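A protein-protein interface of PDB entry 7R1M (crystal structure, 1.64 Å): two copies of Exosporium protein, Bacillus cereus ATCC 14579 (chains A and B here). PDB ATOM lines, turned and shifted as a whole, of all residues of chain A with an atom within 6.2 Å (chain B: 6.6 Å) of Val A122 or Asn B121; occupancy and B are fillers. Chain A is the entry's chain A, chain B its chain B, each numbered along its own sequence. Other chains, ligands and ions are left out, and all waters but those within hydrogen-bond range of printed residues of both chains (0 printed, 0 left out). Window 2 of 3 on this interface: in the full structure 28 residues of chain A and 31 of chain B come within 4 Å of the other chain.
The guanidinium group of Arg A119 lies within hydrogen-bond range of the backbone carbonyl oxygen of Gly B124 (3.2 Å). The side-chain amide nitrogen (ND2) of Asn A121 is in hydrogen-bond range of the backbone carbonyl oxygen (O) of Thr B125. The backbone carbonyl oxygen (O) of Ile B123 sits close to the side-chain amide oxygen (OD1) of Asn A121 (3.3 Å). The guanidinium group (NH1) of Arg A119 sits at hydrogen-bond distance from the backbone carbonyl oxygen (O) of Thr B125, 2.9 Å away. The backbone carbonyl oxygen of Ile B123 sits at hydrogen-bond distance from the guanidinium group of Arg A119.
The guanidinium group of Arg A119 sits at hydrogen-bond distance from the side-chain amide oxygen of Asn A121, at 2.9 Å.
Among the printed residues, pairs that only touch across the chains: Asn A121 with Gly B124, Val A122 with Asn B121, Val A122 with Val B122, Val A122 with Gly B124 and Ile A123 with Val B122.
Of the printed residues of chain B, Val A122 touches Asn B121 (3.7 Å), Val B122 (3.3 Å) and Gly B124 (3.5 Å). Printed residues of chain B within 4 Å of Ile A123: Val B122 (3.5 Å). Leu B88 touches none of the printed residues of chain A. Pro B95 touches none of the printed residues of chain A. Of chain A, only Val A122 comes within 4 Å of Asn B121. Printed residues of chain A within 4 Å of Val B122: Val A122 (3.3 Å) and Ile A123 (3.5 Å). Of the printed residues of chain A, Gly B124 touches Arg A119, Asn A121 and Val A122. Of the printed residues of chain A, Thr B125 touches Arg A119 (2.9 Å) and Asn A121 (3.3 Å). The nearest residue of chain B that does not touch Val A122 is Ile B123 (4.03 Å). The nearest printed residue of chain A that does not touch Asn B121 is Ile A123 (7.1 Å). The nearest printed residue of chain A that does not touch Ile B123 is Val A122 (4.03 Å).
Hydrophobic or aromatic side chains of chain B within 4 Å of the printed part of chain A: Ile B123. Of the 6 printed residues of chain A, 4 touch a printed residue of chain B. Hydrophobic or aromatic side chains of chain A within 4 Å of the printed part of chain B: Val A122 and Ile A123.
Asn A121 touches Gly B124, but with the chains exchanged Gly A124 does not touch Asn B121 (9.3 Å). Val A122 touches Asn B121, but with the chains exchanged Asn A121 does not touch Val B122 (6.7 Å). Val A122 touches its own counterpart, Val B122. Ile A123 touches Val B122, but with the chains exchanged Val A122 does not touch Ile B123 (4.03 Å). Of the 10 pairs that touch across the chains among the printed residues, 1 has its exchanged pair printed and touching as well.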
ATOM      1  N   ARG A 119      -9.823 -22.411 -12.462  1.00  0.00           N
ATOM      2  CA  ARG A 119     -10.746 -21.323 -12.072  1.00  0.00           C
ATOM      3  C   ARG A 119     -11.505 -21.812 -10.840  1.00  0.00           C
ATOM      4  O   ARG A 119     -11.868 -22.986 -10.816  1.00  0.00           O
ATOM      5  CB  ARG A 119     -11.747 -21.011 -13.185  1.00  0.00           C
ATOM      6  CG  ARG A 119     -11.156 -20.479 -14.480  1.00  0.00           C
ATOM      7  CD  ARG A 119     -12.211 -20.214 -15.538  1.00  0.00           C
ATOM      8  NE  ARG A 119     -12.563 -21.370 -16.353  1.00  0.00           N
ATOM      9  CZ  ARG A 119     -13.566 -22.204 -16.100  1.00  0.00           C
ATOM     10  NH1 ARG A 119     -14.332 -22.018 -15.041  1.00  0.00           N
ATOM     11  NH2 ARG A 119     -13.808 -23.216 -16.911  1.00  0.00           N
ATOM     12  N   SER A 120     -11.739 -20.930  -9.873  1.00  0.00           N
ATOM     13  CA  SER A 120     -12.440 -21.282  -8.614  1.00  0.00           C
ATOM     14  C   SER A 120     -13.946 -21.048  -8.729  1.00  0.00           C
ATOM     15  O   SER A 120     -14.648 -21.378  -7.767  1.00  0.00           O
ATOM     16  CB  SER A 120     -11.918 -20.405  -7.526  1.00  0.00           C
ATOM     17  OG  SER A 120     -12.225 -19.052  -7.797  1.00  0.00           O
ATOM     18  N   ASN A 121     -14.436 -20.587  -9.871  1.00  0.00           N
ATOM     19  CA  ASN A 121     -15.860 -20.159  -9.948  1.00  0.00           C
ATOM     20  C   ASN A 121     -16.867 -21.260  -9.591  1.00  0.00           C
ATOM     21  O   ASN A 121     -17.828 -20.923  -8.884  1.00  0.00           O
ATOM     22  CB  ASN A 121     -16.172 -19.427 -11.253  1.00  0.00           C
ATOM     23  CG  ASN A 121     -15.946 -20.260 -12.497  1.00  0.00           C
ATOM     24  OD1 ASN A 121     -15.278 -21.289 -12.451  1.00  0.00           O
ATOM     25  ND2 ASN A 121     -16.501 -19.822 -13.616  1.00  0.00           N
ATOM     26  N   VAL A 122     -16.707 -22.498 -10.053  1.00  0.00           N
ATOM     27  CA  VAL A 122     -17.768 -23.497  -9.710  1.00  0.00           C
ATOM     28  C   VAL A 122     -17.188 -24.659  -8.894  1.00  0.00           C
ATOM     29  O   VAL A 122     -17.919 -25.215  -8.063  1.00  0.00           O
ATOM     30  CB  VAL A 122     -18.553 -23.944 -10.959  1.00  0.00           C
ATOM     31  CG1 VAL A 122     -19.521 -25.077 -10.669  1.00  0.00           C
ATOM     32  CG2 VAL A 122     -19.300 -22.781 -11.590  1.00  0.00           C
ATOM     33  N   ILE A 123     -15.903 -24.955  -9.057  1.00  0.00           N
ATOM     34  CA  ILE A 123     -15.262 -26.106  -8.356  1.00  0.00           C
ATOM     35  C   ILE A 123     -15.370 -25.864  -6.852  1.00  0.00           C
ATOM     36  O   ILE A 123     -15.653 -26.826  -6.117  1.00  0.00           O
ATOM     37  CB  ILE A 123     -13.791 -26.222  -8.805  1.00  0.00           C
ATOM     38  CG1 ILE A 123     -13.686 -26.631 -10.276  1.00  0.00           C
ATOM     39  CG2 ILE A 123     -13.004 -27.157  -7.901  1.00  0.00           C
ATOM     40  CD1 ILE A 123     -14.447 -27.885 -10.617  1.00  0.00           C
ATOM     41  N   GLY A 124     -15.161 -24.623  -6.421  1.00  0.00           N
ATOM     42  CA  GLY A 124     -15.329 -24.285  -4.999  1.00  0.00           C
ATOM     43  C   GLY A 124     -14.033 -24.207  -4.217  1.00  0.00           C
ATOM     44  O   GLY A 124     -13.267 -23.260  -4.456  1.00  0.00           O
ATOM     45  N   LEU B  88     -16.143 -22.081 -22.850  1.00  0.00           N
ATOM     46  CA  LEU B  88     -17.504 -22.339 -22.302  1.00  0.00           C
ATOM     47  C   LEU B  88     -18.143 -21.004 -21.945  1.00  0.00           C
ATOM     48  O   LEU B  88     -17.495 -20.190 -21.255  1.00  0.00           O
ATOM     49  CB  LEU B  88     -17.423 -23.251 -21.080  1.00  0.00           C
ATOM     50  CG  LEU B  88     -16.802 -24.630 -21.319  1.00  0.00           C
ATOM     51  CD1 LEU B  88     -16.641 -25.350 -20.004  1.00  0.00           C
ATOM     52  CD2 LEU B  88     -17.567 -25.471 -22.333  1.00  0.00           C
ATOM     53  N   ASN B  90     -22.112 -20.901 -22.024  1.00  0.00           N
ATOM     54  CA  ASN B  90     -23.541 -21.197 -21.717  1.00  0.00           C
ATOM     55  C   ASN B  90     -24.414 -20.355 -22.668  1.00  0.00           C
ATOM     56  O   ASN B  90     -25.590 -20.129 -22.323  1.00  0.00           O
ATOM     57  CB  ASN B  90     -23.860 -20.978 -20.229  1.00  0.00           C
ATOM     58  CG  ASN B  90     -23.434 -22.142 -19.359  1.00  0.00           C
ATOM     59  OD1 ASN B  90     -23.127 -23.219 -19.889  1.00  0.00           O
ATOM     60  ND2 ASN B  90     -23.395 -21.933 -18.052  1.00  0.00           N
ATOM     61  N   ALA B  94     -27.310 -23.858 -22.878  1.00  0.00           N
ATOM     62  CA  ALA B  94     -26.668 -24.191 -21.589  1.00  0.00           C
ATOM     63  C   ALA B  94     -27.246 -25.506 -21.075  1.00  0.00           C
ATOM     64  O   ALA B  94     -28.402 -25.826 -21.362  1.00  0.00           O
ATOM     65  CB  ALA B  94     -26.871 -23.084 -20.600  1.00  0.00           C
ATOM     66  N   PRO B  95     -26.443 -26.368 -20.413  1.00  0.00           N
ATOM     67  CA  PRO B  95     -24.988 -26.182 -20.282  1.00  0.00           C
ATOM     68  C   PRO B  95     -24.254 -26.506 -21.594  1.00  0.00           C
ATOM     69  O   PRO B  95     -24.862 -26.848 -22.600  1.00  0.00           O
ATOM     70  CB  PRO B  95     -24.683 -27.150 -19.139  1.00  0.00           C
ATOM     71  CG  PRO B  95     -25.597 -28.316 -19.432  1.00  0.00           C
ATOM     72  CD  PRO B  95     -26.902 -27.628 -19.801  1.00  0.00           C
ATOM     73  N   GLU B  96     -22.960 -26.222 -21.648  1.00  0.00           N
ATOM     74  CA  GLU B  96     -22.110 -26.638 -22.777  1.00  0.00           C
ATOM     75  C   GLU B  96     -21.222 -27.759 -22.245  1.00  0.00           C
ATOM     76  O   GLU B  96     -20.705 -27.634 -21.106  1.00  0.00           O
ATOM     77  CB  GLU B  96     -21.288 -25.479 -23.333  1.00  0.00           C
ATOM     78  CG  GLU B  96     -22.099 -24.506 -24.172  1.00  0.00           C
ATOM     79  CD  GLU B  96     -21.383 -23.211 -24.483  1.00  0.00           C
ATOM     80  OE1 GLU B  96     -20.468 -22.848 -23.684  1.00  0.00           O
ATOM     81  OE2 GLU B  96     -21.727 -22.567 -25.496  1.00  0.00           O
ATOM     82  N   ARG B 119     -17.616 -30.092 -18.826  1.00  0.00           N
ATOM     83  CA  ARG B 119     -19.026 -29.901 -18.438  1.00  0.00           C
ATOM     84  C   ARG B 119     -19.151 -28.564 -17.726  1.00  0.00           C
ATOM     85  O   ARG B 119     -18.660 -28.462 -16.604  1.00  0.00           O
ATOM     86  CB  ARG B 119     -19.473 -31.071 -17.576  1.00  0.00           C
ATOM     87  CG  ARG B 119     -19.256 -32.407 -18.257  1.00  0.00           C
ATOM     88  CD  ARG B 119     -20.081 -33.528 -17.702  1.00  0.00           C
ATOM     89  NE  ARG B 119     -19.770 -34.768 -18.399  1.00  0.00           N
ATOM     90  CZ  ARG B 119     -20.376 -35.242 -19.494  1.00  0.00           C
ATOM     91  NH1 ARG B 119     -19.971 -36.397 -19.995  1.00  0.00           N
ATOM     92  NH2 ARG B 119     -21.374 -34.587 -20.084  1.00  0.00           N
ATOM     93  N   SER B 120     -19.779 -27.574 -18.368  1.00  0.00           N
ATOM     94  CA  SER B 120     -19.850 -26.216 -17.792  1.00  0.00           C
ATOM     95  C   SER B 120     -20.553 -26.224 -16.426  1.00  0.00           C
ATOM     96  O   SER B 120     -20.223 -25.369 -15.618  1.00  0.00           O
ATOM     97  CB  SER B 120     -20.482 -25.256 -18.738  1.00  0.00           C
ATOM     98  OG  SER B 120     -21.871 -25.507 -18.856  1.00  0.00           O
ATOM     99  N   ASN B 121     -21.481 -27.131 -16.122  1.00  0.00           N
ATOM    100  CA  ASN B 121     -22.132 -27.122 -14.789  1.00  0.00           C
ATOM    101  C   ASN B 121     -21.192 -27.702 -13.740  1.00  0.00           C
ATOM    102  O   ASN B 121     -21.465 -27.510 -12.577  1.00  0.00           O
ATOM    103  CB  ASN B 121     -23.422 -27.942 -14.704  1.00  0.00           C
ATOM    104  CG  ASN B 121     -24.588 -27.255 -15.383  1.00  0.00           C
ATOM    105  OD1 ASN B 121     -24.537 -26.056 -15.633  1.00  0.00           O
ATOM    106  ND2 ASN B 121     -25.636 -28.015 -15.684  1.00  0.00           N
ATOM    107  N   VAL B 122     -20.132 -28.398 -14.146  1.00  0.00           N
ATOM    108  CA  VAL B 122     -19.110 -28.922 -13.195  1.00  0.00           C
ATOM    109  C   VAL B 122     -18.006 -27.881 -13.028  1.00  0.00           C
ATOM    110  O   VAL B 122     -17.657 -27.539 -11.865  1.00  0.00           O
ATOM    111  CB  VAL B 122     -18.567 -30.290 -13.664  1.00  0.00           C
ATOM    112  CG1 VAL B 122     -17.473 -30.805 -12.722  1.00  0.00           C
ATOM    113  CG2 VAL B 122     -19.675 -31.317 -13.813  1.00  0.00           C
ATOM    114  N   ILE B 123     -17.478 -27.362 -14.128  1.00  0.00           N
ATOM    115  CA  ILE B 123     -16.213 -26.569 -14.076  1.00  0.00           C
ATOM    116  C   ILE B 123     -16.512 -25.078 -14.240  1.00  0.00           C
ATOM    117  O   ILE B 123     -15.626 -24.275 -13.914  1.00  0.00           O
ATOM    118  CB  ILE B 123     -15.154 -27.136 -15.056  1.00  0.00           C
ATOM    119  CG1 ILE B 123     -13.742 -26.730 -14.607  1.00  0.00           C
ATOM    120  CG2 ILE B 123     -15.416 -26.776 -16.513  1.00  0.00           C
ATOM    121  CD1 ILE B 123     -12.634 -27.463 -15.297  1.00  0.00           C
ATOM    122  N   GLY B 124     -17.734 -24.685 -14.622  1.00  0.00           N
ATOM    123  CA  GLY B 124     -18.068 -23.262 -14.818  1.00  0.00           C
ATOM    124  C   GLY B 124     -17.649 -22.735 -16.175  1.00  0.00           C
ATOM    125  O   GLY B 124     -16.995 -23.429 -16.933  1.00  0.00           O
ATOM    126  N   THR B 125     -18.050 -21.521 -16.506  1.00  0.00           N
ATOM    127  CA  THR B 125     -17.765 -20.905 -17.826  1.00  0.00           C
ATOM    128  C   THR B 125     -16.326 -20.347 -17.864  1.00  0.00           C
ATOM    129  O   THR B 125     -15.705 -20.216 -16.794  1.00  0.00           O
ATOM    130  CB  THR B 125     -18.817 -19.838 -18.137  1.00  0.00           C
ATOM    131  OG1 THR B 125     -18.763 -18.922 -17.051  1.00  0.00           O
ATOM    132  CG2 THR B 125     -20.205 -20.405 -18.323  1.00  0.00           C
